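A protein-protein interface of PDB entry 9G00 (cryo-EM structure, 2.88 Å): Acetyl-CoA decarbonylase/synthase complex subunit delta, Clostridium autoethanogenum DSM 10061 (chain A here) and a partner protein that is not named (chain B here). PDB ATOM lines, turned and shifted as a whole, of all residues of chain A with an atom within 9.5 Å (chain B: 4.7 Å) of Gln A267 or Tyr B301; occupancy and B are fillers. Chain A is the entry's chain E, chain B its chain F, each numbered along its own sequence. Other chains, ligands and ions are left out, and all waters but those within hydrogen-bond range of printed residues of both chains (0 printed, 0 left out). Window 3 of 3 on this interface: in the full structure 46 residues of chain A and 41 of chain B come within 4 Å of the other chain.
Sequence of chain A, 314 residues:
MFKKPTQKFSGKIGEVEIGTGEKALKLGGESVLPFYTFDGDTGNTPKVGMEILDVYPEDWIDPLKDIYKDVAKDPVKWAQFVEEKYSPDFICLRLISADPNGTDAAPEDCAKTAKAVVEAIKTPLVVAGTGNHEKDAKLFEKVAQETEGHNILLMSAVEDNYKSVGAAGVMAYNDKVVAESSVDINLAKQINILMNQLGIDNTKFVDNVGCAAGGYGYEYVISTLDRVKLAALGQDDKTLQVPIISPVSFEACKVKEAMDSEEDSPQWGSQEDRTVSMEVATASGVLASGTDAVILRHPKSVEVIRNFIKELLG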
ATOM      1  N   LYS A 256     -10.751  -2.222 -15.462  1.00  0.00           N
ATOM      2  CA  LYS A 256     -11.725  -3.268 -15.752  1.00  0.00           C
ATOM      3  C   LYS A 256     -11.159  -4.646 -15.446  1.00  0.00           C
ATOM      4  O   LYS A 256     -11.875  -5.528 -14.961  1.00  0.00           O
ATOM      5  CB  LYS A 256     -12.153  -3.184 -17.217  1.00  0.00           C
ATOM      6  CG  LYS A 256     -13.252  -4.162 -17.611  1.00  0.00           C
ATOM      7  CD  LYS A 256     -13.581  -4.048 -19.093  1.00  0.00           C
ATOM      8  CE  LYS A 256     -14.802  -4.875 -19.470  1.00  0.00           C
ATOM      9  NZ  LYS A 256     -14.629  -6.314 -19.141  1.00  0.00           N
ATOM     10  N   GLU A 257      -9.877  -4.852 -15.736  1.00  0.00           N
ATOM     11  CA  GLU A 257      -9.247  -6.149 -15.553  1.00  0.00           C
ATOM     12  C   GLU A 257      -9.105  -6.541 -14.092  1.00  0.00           C
ATOM     13  O   GLU A 257      -8.846  -7.714 -13.808  1.00  0.00           O
ATOM     14  CB  GLU A 257      -7.879  -6.143 -16.226  1.00  0.00           C
ATOM     15  CG  GLU A 257      -7.937  -5.737 -17.685  1.00  0.00           C
ATOM     16  CD  GLU A 257      -6.590  -5.352 -18.235  1.00  0.00           C
ATOM     17  OE1 GLU A 257      -5.601  -5.381 -17.472  1.00  0.00           O
ATOM     18  OE2 GLU A 257      -6.519  -5.014 -19.434  1.00  0.00           O
ATOM     19  N   ALA A 258      -9.266  -5.597 -13.162  1.00  0.00           N
ATOM     20  CA  ALA A 258      -9.136  -5.882 -11.743  1.00  0.00           C
ATOM     21  C   ALA A 258     -10.446  -5.787 -10.976  1.00  0.00           C
ATOM     22  O   ALA A 258     -10.559  -6.399  -9.912  1.00  0.00           O
ATOM     23  CB  ALA A 258      -8.120  -4.927 -11.102  1.00  0.00           C
ATOM     24  N   ASP A 260     -13.754  -6.265 -12.506  1.00  0.00           N
ATOM     25  CA  ASP A 260     -14.797  -7.155 -12.998  1.00  0.00           C
ATOM     26  C   ASP A 260     -14.808  -8.449 -12.198  1.00  0.00           C
ATOM     27  O   ASP A 260     -13.760  -9.051 -11.953  1.00  0.00           O
ATOM     28  CB  ASP A 260     -14.587  -7.454 -14.480  1.00  0.00           C
ATOM     29  CG  ASP A 260     -15.174  -6.389 -15.375  1.00  0.00           C
ATOM     30  OD1 ASP A 260     -15.685  -5.383 -14.842  1.00  0.00           O
ATOM     31  OD2 ASP A 260     -15.130  -6.556 -16.611  1.00  0.00           O
ATOM     32  N   SER A 261     -16.001  -8.870 -11.789  1.00  0.00           N
ATOM     33  CA  SER A 261     -16.167 -10.104 -11.045  1.00  0.00           C
ATOM     34  C   SER A 261     -16.388 -11.260 -12.016  1.00  0.00           C
ATOM     35  O   SER A 261     -16.407 -11.086 -13.236  1.00  0.00           O
ATOM     36  CB  SER A 261     -17.321  -9.973 -10.053  1.00  0.00           C
ATOM     37  OG  SER A 261     -18.514  -9.574 -10.703  1.00  0.00           O
ATOM     38  N   GLU A 262     -16.563 -12.464 -11.469  1.00  0.00           N
ATOM     39  CA  GLU A 262     -16.772 -13.628 -12.323  1.00  0.00           C
ATOM     40  C   GLU A 262     -18.091 -13.542 -13.081  1.00  0.00           C
ATOM     41  O   GLU A 262     -18.194 -14.057 -14.199  1.00  0.00           O
ATOM     42  CB  GLU A 262     -16.719 -14.909 -11.494  1.00  0.00           C
ATOM     43  CG  GLU A 262     -15.395 -15.115 -10.783  1.00  0.00           C
ATOM     44  CD  GLU A 262     -15.140 -16.563 -10.414  1.00  0.00           C
ATOM     45  OE1 GLU A 262     -15.796 -17.453 -10.994  1.00  0.00           O
ATOM     46  OE2 GLU A 262     -14.280 -16.814  -9.543  1.00  0.00           O
ATOM     47  N   GLU A 263     -19.104 -12.896 -12.500  1.00  0.00           N
ATOM     48  CA  GLU A 263     -20.375 -12.756 -13.200  1.00  0.00           C
ATOM     49  C   GLU A 263     -20.206 -11.943 -14.476  1.00  0.00           C
ATOM     50  O   GLU A 263     -20.764 -12.291 -15.523  1.00  0.00           O
ATOM     51  CB  GLU A 263     -21.417 -12.106 -12.288  1.00  0.00           C
ATOM     52  CG  GLU A 263     -21.788 -12.928 -11.062  1.00  0.00           C
ATOM     53  CD  GLU A 263     -20.773 -12.805  -9.941  1.00  0.00           C
ATOM     54  OE1 GLU A 263     -19.796 -12.044 -10.104  1.00  0.00           O
ATOM     55  OE2 GLU A 263     -20.950 -13.468  -8.899  1.00  0.00           O
ATOM     56  N   ASP A 264     -19.445 -10.849 -14.408  1.00  0.00           N
ATOM     57  CA  ASP A 264     -19.250 -10.007 -15.583  1.00  0.00           C
ATOM     58  C   ASP A 264     -18.364 -10.692 -16.617  1.00  0.00           C
ATOM     59  O   ASP A 264     -18.694 -10.723 -17.808  1.00  0.00           O
ATOM     60  CB  ASP A 264     -18.642  -8.670 -15.168  1.00  0.00           C
ATOM     61  CG  ASP A 264     -19.506  -7.922 -14.182  1.00  0.00           C
ATOM     62  OD1 ASP A 264     -19.748  -8.454 -13.080  1.00  0.00           O
ATOM     63  OD2 ASP A 264     -19.940  -6.799 -14.509  1.00  0.00           O
ATOM     64  N   SER A 265     -17.236 -11.251 -16.182  1.00  0.00           N
ATOM     65  CA  SER A 265     -16.264 -11.878 -17.077  1.00  0.00           C
ATOM     66  C   SER A 265     -15.940 -13.270 -16.554  1.00  0.00           C
ATOM     67  O   SER A 265     -14.956 -13.459 -15.827  1.00  0.00           O
ATOM     68  CB  SER A 265     -15.000 -11.032 -17.194  1.00  0.00           C
ATOM     69  OG  SER A 265     -15.291  -9.763 -17.749  1.00  0.00           O
ATOM     70  N   PRO A 266     -16.747 -14.273 -16.905  1.00  0.00           N
ATOM     71  CA  PRO A 266     -16.480 -15.627 -16.394  1.00  0.00           C
ATOM     72  C   PRO A 266     -15.132 -16.186 -16.815  1.00  0.00           C
ATOM     73  O   PRO A 266     -14.523 -16.943 -16.048  1.00  0.00           O
ATOM     74  CB  PRO A 266     -17.641 -16.451 -16.970  1.00  0.00           C
ATOM     75  CG  PRO A 266     -18.086 -15.693 -18.171  1.00  0.00           C
ATOM     76  CD  PRO A 266     -17.892 -14.249 -17.830  1.00  0.00           C
ATOM     77  N   GLN A 267     -14.646 -15.840 -18.010  1.00  0.00           N
ATOM     78  CA  GLN A 267     -13.404 -16.430 -18.498  1.00  0.00           C
ATOM     79  C   GLN A 267     -12.180 -15.898 -17.762  1.00  0.00           C
ATOM     80  O   GLN A 267     -11.162 -16.594 -17.680  1.00  0.00           O
ATOM     81  CB  GLN A 267     -13.259 -16.184 -20.004  1.00  0.00           C
ATOM     82  CG  GLN A 267     -13.011 -14.731 -20.417  1.00  0.00           C
ATOM     83  CD  GLN A 267     -14.273 -13.891 -20.423  1.00  0.00           C
ATOM     84  OE1 GLN A 267     -15.359 -14.382 -20.117  1.00  0.00           O
ATOM     85  NE2 GLN A 267     -14.136 -12.618 -20.774  1.00  0.00           N
ATOM     86  N   TRP A 268     -12.260 -14.691 -17.199  1.00  0.00           N
ATOM     87  CA  TRP A 268     -11.104 -14.085 -16.546  1.00  0.00           C
ATOM     88  C   TRP A 268     -10.756 -14.731 -15.213  1.00  0.00           C
ATOM     89  O   TRP A 268      -9.702 -14.415 -14.654  1.00  0.00           O
ATOM     90  CB  TRP A 268     -11.344 -12.589 -16.347  1.00  0.00           C
ATOM     91  CG  TRP A 268     -11.106 -11.768 -17.578  1.00  0.00           C
ATOM     92  CD1 TRP A 268     -10.666 -12.211 -18.789  1.00  0.00           C
ATOM     93  CD2 TRP A 268     -11.291 -10.356 -17.712  1.00  0.00           C
ATOM     94  NE1 TRP A 268     -10.567 -11.164 -19.670  1.00  0.00           N
ATOM     95  CE2 TRP A 268     -10.945 -10.013 -19.032  1.00  0.00           C
ATOM     96  CE3 TRP A 268     -11.719  -9.348 -16.845  1.00  0.00           C
ATOM     97  CZ2 TRP A 268     -11.013  -8.708 -19.504  1.00  0.00           C
ATOM     98  CZ3 TRP A 268     -11.785  -8.057 -17.316  1.00  0.00           C
ATOM     99  CH2 TRP A 268     -11.434  -7.747 -18.632  1.00  0.00           C
ATOM    100  N   GLY A 269     -11.603 -15.609 -14.685  1.00  0.00           N
ATOM    101  CA  GLY A 269     -11.280 -16.291 -13.448  1.00  0.00           C
ATOM    102  C   GLY A 269     -11.631 -15.477 -12.212  1.00  0.00           C
ATOM    103  O   GLY A 269     -12.536 -14.644 -12.221  1.00  0.00           O
ATOM    104  N   SER A 270     -10.878 -15.712 -11.143  1.00  0.00           N
ATOM    105  CA  SER A 270     -11.175 -15.085  -9.865  1.00  0.00           C
ATOM    106  C   SER A 270     -10.995 -13.574  -9.941  1.00  0.00           C
ATOM    107  O   SER A 270     -10.253 -13.053 -10.776  1.00  0.00           O
ATOM    108  CB  SER A 270     -10.272 -15.659  -8.774  1.00  0.00           C
ATOM    109  OG  SER A 270     -10.460 -14.987  -7.542  1.00  0.00           O
ATOM    110  N   GLN A 271     -11.705 -12.868  -9.063  1.00  0.00           N
ATOM    111  CA  GLN A 271     -11.596 -11.419  -8.980  1.00  0.00           C
ATOM    112  C   GLN A 271     -10.489 -10.982  -8.032  1.00  0.00           C
ATOM    113  O   GLN A 271      -9.765 -10.025  -8.323  1.00  0.00           O
ATOM    114  CB  GLN A 271     -12.925 -10.814  -8.528  1.00  0.00           C
ATOM    115  CG  GLN A 271     -12.956  -9.299  -8.571  1.00  0.00           C
ATOM    116  CD  GLN A 271     -14.276  -8.743  -8.101  1.00  0.00           C
ATOM    117  OE1 GLN A 271     -14.999  -9.392  -7.350  1.00  0.00           O
ATOM    118  NE2 GLN A 271     -14.604  -7.539  -8.547  1.00  0.00           N
ATOM    119  N   ASP A 273      -7.751 -12.642  -7.267  1.00  0.00           N
ATOM    120  CA  ASP A 273      -6.454 -12.921  -7.875  1.00  0.00           C
ATOM    121  C   ASP A 273      -6.082 -11.848  -8.886  1.00  0.00           C
ATOM    122  O   ASP A 273      -4.925 -11.424  -8.954  1.00  0.00           O
ATOM    123  CB  ASP A 273      -6.468 -14.296  -8.540  1.00  0.00           C
ATOM    124  CG  ASP A 273      -6.324 -15.424  -7.544  1.00  0.00           C
ATOM    125  OD1 ASP A 273      -7.270 -15.652  -6.762  1.00  0.00           O
ATOM    126  OD2 ASP A 273      -5.265 -16.084  -7.541  1.00  0.00           O
ATOM    127  N   ARG A 274      -7.047 -11.404  -9.693  1.00  0.00           N
ATOM    128  CA  ARG A 274      -6.748 -10.382 -10.688  1.00  0.00           C
ATOM    129  C   ARG A 274      -6.487  -9.028 -10.044  1.00  0.00           C
ATOM    130  O   ARG A 274      -5.686  -8.244 -10.563  1.00  0.00           O
ATOM    131  CB  ARG A 274      -7.888 -10.288 -11.699  1.00  0.00           C
ATOM    132  CG  ARG A 274      -7.905 -11.444 -12.677  1.00  0.00           C
ATOM    133  CD  ARG A 274      -8.984 -11.294 -13.720  1.00  0.00           C
ATOM    134  NE  ARG A 274     -10.310 -11.527 -13.162  1.00  0.00           N
ATOM    135  CZ  ARG A 274     -11.157 -10.576 -12.792  1.00  0.00           C
ATOM    136  NH1 ARG A 274     -10.866  -9.294 -12.928  1.00  0.00           N
ATOM    137  NH2 ARG A 274     -12.331 -10.925 -12.275  1.00  0.00           N
ATOM    138  N   THR A 275      -7.153  -8.728  -8.930  1.00  0.00           N
ATOM    139  CA  THR A 275      -6.894  -7.474  -8.230  1.00  0.00           C
ATOM    140  C   THR A 275      -5.498  -7.464  -7.623  1.00  0.00           C
ATOM    141  O   THR A 275      -4.773  -6.469  -7.725  1.00  0.00           O
ATOM    142  CB  THR A 275      -7.958  -7.252  -7.160  1.00  0.00           C
ATOM    143  OG1 THR A 275      -9.230  -7.107  -7.801  1.00  0.00           O
ATOM    144  CG2 THR A 275      -7.661  -6.007  -6.341  1.00  0.00           C
ATOM    145  N   SER A 277      -2.966  -9.447  -8.557  1.00  0.00           N
ATOM    146  CA  SER A 277      -2.000  -9.540  -9.643  1.00  0.00           C
ATOM    147  C   SER A 277      -1.843  -8.215 -10.377  1.00  0.00           C
ATOM    148  O   SER A 277      -0.785  -7.952 -10.956  1.00  0.00           O
ATOM    149  CB  SER A 277      -2.429 -10.638 -10.611  1.00  0.00           C
ATOM    150  OG  SER A 277      -1.544 -10.725 -11.708  1.00  0.00           O
ATOM    151  N   MET A 278      -2.875  -7.374 -10.372  1.00  0.00           N
ATOM    152  CA  MET A 278      -2.774  -6.085 -11.051  1.00  0.00           C
ATOM    153  C   MET A 278      -1.908  -5.110 -10.265  1.00  0.00           C
ATOM    154  O   MET A 278      -1.130  -4.350 -10.852  1.00  0.00           O
ATOM    155  CB  MET A 278      -4.163  -5.497 -11.276  1.00  0.00           C
ATOM    156  CG  MET A 278      -4.221  -4.516 -12.424  1.00  0.00           C
ATOM    157  SD  MET A 278      -3.998  -5.335 -14.011  1.00  0.00           S
ATOM    158  CE  MET A 278      -3.741  -3.931 -15.088  1.00  0.00           C
ATOM    159  N   ASP B 116      -6.712 -22.031 -23.266  1.00  0.00           N
ATOM    160  CA  ASP B 116      -7.785 -21.190 -22.744  1.00  0.00           C
ATOM    161  C   ASP B 116      -7.409 -19.712 -22.791  1.00  0.00           C
ATOM    162  O   ASP B 116      -8.208 -18.874 -23.225  1.00  0.00           O
ATOM    163  CB  ASP B 116      -8.118 -21.624 -21.316  1.00  0.00           C
ATOM    164  CG  ASP B 116      -9.313 -20.893 -20.744  1.00  0.00           C
ATOM    165  OD1 ASP B 116     -10.411 -21.001 -21.328  1.00  0.00           O
ATOM    166  OD2 ASP B 116      -9.157 -20.222 -19.704  1.00  0.00           O
ATOM    167  N   VAL B 117      -6.198 -19.371 -22.354  1.00  0.00           N
ATOM    168  CA  VAL B 117      -5.754 -17.979 -22.284  1.00  0.00           C
ATOM    169  C   VAL B 117      -5.374 -17.548 -23.698  1.00  0.00           C
ATOM    170  O   VAL B 117      -4.271 -17.825 -24.169  1.00  0.00           O
ATOM    171  CB  VAL B 117      -4.590 -17.800 -21.308  1.00  0.00           C
ATOM    172  CG1 VAL B 117      -4.163 -16.343 -21.249  1.00  0.00           C
ATOM    173  CG2 VAL B 117      -4.980 -18.295 -19.930  1.00  0.00           C
ATOM    174  N   ASP B 118      -6.284 -16.855 -24.376  1.00  0.00           N
ATOM    175  CA  ASP B 118      -6.029 -16.383 -25.735  1.00  0.00           C
ATOM    176  C   ASP B 118      -7.009 -15.262 -26.033  1.00  0.00           C
ATOM    177  O   ASP B 118      -8.220 -15.497 -26.070  1.00  0.00           O
ATOM    178  CB  ASP B 118      -6.180 -17.525 -26.736  1.00  0.00           C
ATOM    179  CG  ASP B 118      -5.541 -17.220 -28.072  1.00  0.00           C
ATOM    180  OD1 ASP B 118      -5.542 -16.042 -28.481  1.00  0.00           O
ATOM    181  OD2 ASP B 118      -5.035 -18.164 -28.713  1.00  0.00           O
ATOM    182  N   TYR B 119      -6.493 -14.053 -26.248  1.00  0.00           N
ATOM    183  CA  TYR B 119      -7.336 -12.894 -26.496  1.00  0.00           C
ATOM    184  C   TYR B 119      -6.545 -11.871 -27.296  1.00  0.00           C
ATOM    185  O   TYR B 119      -5.326 -11.978 -27.448  1.00  0.00           O
ATOM    186  CB  TYR B 119      -7.848 -12.287 -25.184  1.00  0.00           C
ATOM    187  CG  TYR B 119      -6.767 -11.733 -24.286  1.00  0.00           C
ATOM    188  CD1 TYR B 119      -6.069 -12.553 -23.412  1.00  0.00           C
ATOM    189  CD2 TYR B 119      -6.451 -10.383 -24.303  1.00  0.00           C
ATOM    190  CE1 TYR B 119      -5.086 -12.046 -22.590  1.00  0.00           C
ATOM    191  CE2 TYR B 119      -5.472  -9.870 -23.486  1.00  0.00           C
ATOM    192  CZ  TYR B 119      -4.793 -10.703 -22.633  1.00  0.00           C
ATOM    193  OH  TYR B 119      -3.819 -10.183 -21.820  1.00  0.00           O
ATOM    194  N   ASP B 300      -2.463 -18.259 -16.623  1.00  0.00           N
ATOM    195  CA  ASP B 300      -3.865 -17.999 -16.334  1.00  0.00           C
ATOM    196  C   ASP B 300      -4.106 -16.509 -16.505  1.00  0.00           C
ATOM    197  O   ASP B 300      -3.169 -15.714 -16.593  1.00  0.00           O
ATOM    198  CB  ASP B 300      -4.244 -18.470 -14.930  1.00  0.00           C
ATOM    199  CG  ASP B 300      -3.300 -17.956 -13.876  1.00  0.00           C
ATOM    200  OD1 ASP B 300      -2.102 -17.807 -14.189  1.00  0.00           O
ATOM    201  OD2 ASP B 300      -3.752 -17.698 -12.742  1.00  0.00           O
ATOM    202  N   TYR B 301      -5.384 -16.137 -16.557  1.00  0.00           N
ATOM    203  CA  TYR B 301      -5.730 -14.741 -16.794  1.00  0.00           C
ATOM    204  C   TYR B 301      -5.258 -13.825 -15.676  1.00  0.00           C
ATOM    205  O   TYR B 301      -5.126 -12.617 -15.898  1.00  0.00           O
ATOM    206  CB  TYR B 301      -7.234 -14.599 -16.981  1.00  0.00           C
ATOM    207  CG  TYR B 301      -7.687 -14.903 -18.385  1.00  0.00           C
ATOM    208  CD1 TYR B 301      -7.618 -13.939 -19.377  1.00  0.00           C
ATOM    209  CD2 TYR B 301      -8.182 -16.151 -18.720  1.00  0.00           C
ATOM    210  CE1 TYR B 301      -8.030 -14.208 -20.656  1.00  0.00           C
ATOM    211  CE2 TYR B 301      -8.596 -16.428 -19.998  1.00  0.00           C
ATOM    212  CZ  TYR B 301      -8.519 -15.452 -20.962  1.00  0.00           C
ATOM    213  OH  TYR B 301      -8.932 -15.724 -22.241  1.00  0.00           O
ATOM    214  N   SER B 302      -5.014 -14.360 -14.481  1.00  0.00           N
ATOM    215  CA  SER B 302      -4.447 -13.540 -13.415  1.00  0.00           C
ATOM    216  C   SER B 302      -3.044 -13.074 -13.780  1.00  0.00           C
ATOM    217  O   SER B 302      -2.682 -11.919 -13.528  1.00  0.00           O
ATOM    218  CB  SER B 302      -4.432 -14.315 -12.103  1.00  0.00           C
ATOM    219  OG  SER B 302      -3.585 -15.441 -12.193  1.00  0.00           O
ATOM    220  N   ARG B 303      -2.238 -13.959 -14.368  1.00  0.00           N
ATOM    221  CA  ARG B 303      -0.919 -13.568 -14.851  1.00  0.00           C
ATOM    222  C   ARG B 303      -1.007 -12.842 -16.186  1.00  0.00           C
ATOM    223  O   ARG B 303      -0.305 -11.850 -16.403  1.00  0.00           O
ATOM    224  CB  ARG B 303      -0.021 -14.794 -15.012  1.00  0.00           C
ATOM    225  CG  ARG B 303       0.230 -15.598 -13.759  1.00  0.00           C
ATOM    226  CD  ARG B 303       1.196 -16.738 -14.059  1.00  0.00           C
ATOM    227  NE  ARG B 303       1.477 -17.568 -12.893  1.00  0.00           N
ATOM    228  CZ  ARG B 303       0.809 -18.667 -12.571  1.00  0.00           C
ATOM    229  NH1 ARG B 303      -0.205 -19.103 -13.300  1.00  0.00           N
ATOM    230  NH2 ARG B 303       1.166 -19.349 -11.487  1.00  0.00           N
ATOM    231  N   ALA B 304      -1.854 -13.324 -17.094  1.00  0.00           N
ATOM    232  CA  ALA B 304      -1.824 -12.838 -18.469  1.00  0.00           C
ATOM    233  C   ALA B 304      -2.242 -11.377 -18.561  1.00  0.00           C
ATOM    234  O   ALA B 304      -1.613 -10.595 -19.281  1.00  0.00           O
ATOM    235  CB  ALA B 304      -2.722 -13.703 -19.349  1.00  0.00           C
ATOM    236  N   LEU B 305      -3.296 -10.987 -17.852  1.00  0.00           N
ATOM    237  CA  LEU B 305      -3.840  -9.643 -18.037  1.00  0.00           C
ATOM    238  C   LEU B 305      -2.835  -8.554 -17.695  1.00  0.00           C
ATOM    239  O   LEU B 305      -2.681  -7.618 -18.500  1.00  0.00           O
ATOM    240  CB  LEU B 305      -5.136  -9.494 -17.234  1.00  0.00           C
ATOM    241  CG  LEU B 305      -6.337 -10.279 -17.767  1.00  0.00           C
ATOM    242  CD1 LEU B 305      -7.510 -10.140 -16.825  1.00  0.00           C
ATOM    243  CD2 LEU B 305      -6.734  -9.824 -19.161  1.00  0.00           C
ATOM    244  N   PRO B 306      -2.133  -8.586 -16.560  1.00  0.00           N
ATOM    245  CA  PRO B 306      -1.130  -7.536 -16.325  1.00  0.00           C
ATOM    246  C   PRO B 306       0.117  -7.695 -17.176  1.00  0.00           C
ATOM    247  O   PRO B 306       0.612  -6.706 -17.729  1.00  0.00           O
ATOM    248  CB  PRO B 306      -0.811  -7.679 -14.830  1.00  0.00           C
ATOM    249  CG  PRO B 306      -1.864  -8.564 -14.276  1.00  0.00           C
ATOM    250  CD  PRO B 306      -2.286  -9.451 -15.382  1.00  0.00           C
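The side-chain hydroxyl of Ser A277 is in hydrogen-bond range of the backbone carbonyl oxygen of Ser B302.
NH1 of Arg A274 is in hydrogen-bond range of O of Glu A257. The guanidinium group (NH1) of Arg A274 is in hydrogen-bond range of the backbone carbonyl oxygen (O) of Asp A260, at 3.1 Å. The guanidinium group (NE) of Arg A274 sits at hydrogen-bond distance from the backbone carbonyl oxygen (O) of Trp A268. NE of Arg A274 is in hydrogen-bond range of O of Ser A270 (2.8 Å). The backbone carbonyl oxygen (O) of Asp B116 is in hydrogen-bond range of the side-chain hydroxyl (OH) of Tyr B301, at 3.4 Å. The side-chain hydroxyl (OG) of Ser B302 sits close to the side-chain carboxylate (OD1) of Asp B300 (3.4 Å).
Leu B305 touches Glu A257. Gln A267 touches Tyr B301. Trp A268 touches Tyr B301. Trp A268 touches Leu B305 (CD2 to CD1, 3.9 Å). CD1 of Leu B305 touches CD of Arg A274 (3.6 Å). Ser A277 touches Pro B306 (OG to CG, 3.4 Å). SD of Met A278 touches CG of Pro B306, 3.9 Å away.
Gln A267 touches just one residue of chain B: Tyr B301. Tyr B301 touches just these residues of chain A: Gln A267 and Trp A268. Ser B302 touches just one residue of chain A: Ser A277. No residue of chain A comes within 4 Å of Ala B304. Printed residues of chain B within 4 Å of Glu A257: Leu B305. Printed residues of chain B within 4 Å of Trp A268: Tyr B301 and Leu B305. Printed residues of chain A within 4 Å of Pro B306: Ser A277 and Met A278. Of the printed residues of chain A, Leu B305 touches Glu A257 (3.8 Å), Trp A268 (3.9 Å) and Arg A274 (3.6 Å). Of the printed residues of chain B, Met A278 touches Pro B306. Glu A262 touches none of the printed residues of chain B. The nearest residue of chain B that does not touch Gln A267 is Asp B116 (4.6 Å). The nearest residue of chain A that does not touch Tyr B301 is Arg A274 (4.4 Å).
Of the 11 printed residues of chain B, 4 touch a printed residue of chain A. Hydrophobic or aromatic side chains of chain B within 4 Å of the printed part of chain A: Tyr B301, Leu B305 and Pro B306. Of the 20 printed residues of chain A, 6 touch a printed residue of chain B. Hydrophobic or aromatic side chains of chain A within 4 Å of the printed part of chain B: Trp A268 and Met A278. Among the printed residues, no Asp or Glu carboxylate lies within 4 Å of a Lys or Arg side-chain nitrogen of the other chain.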
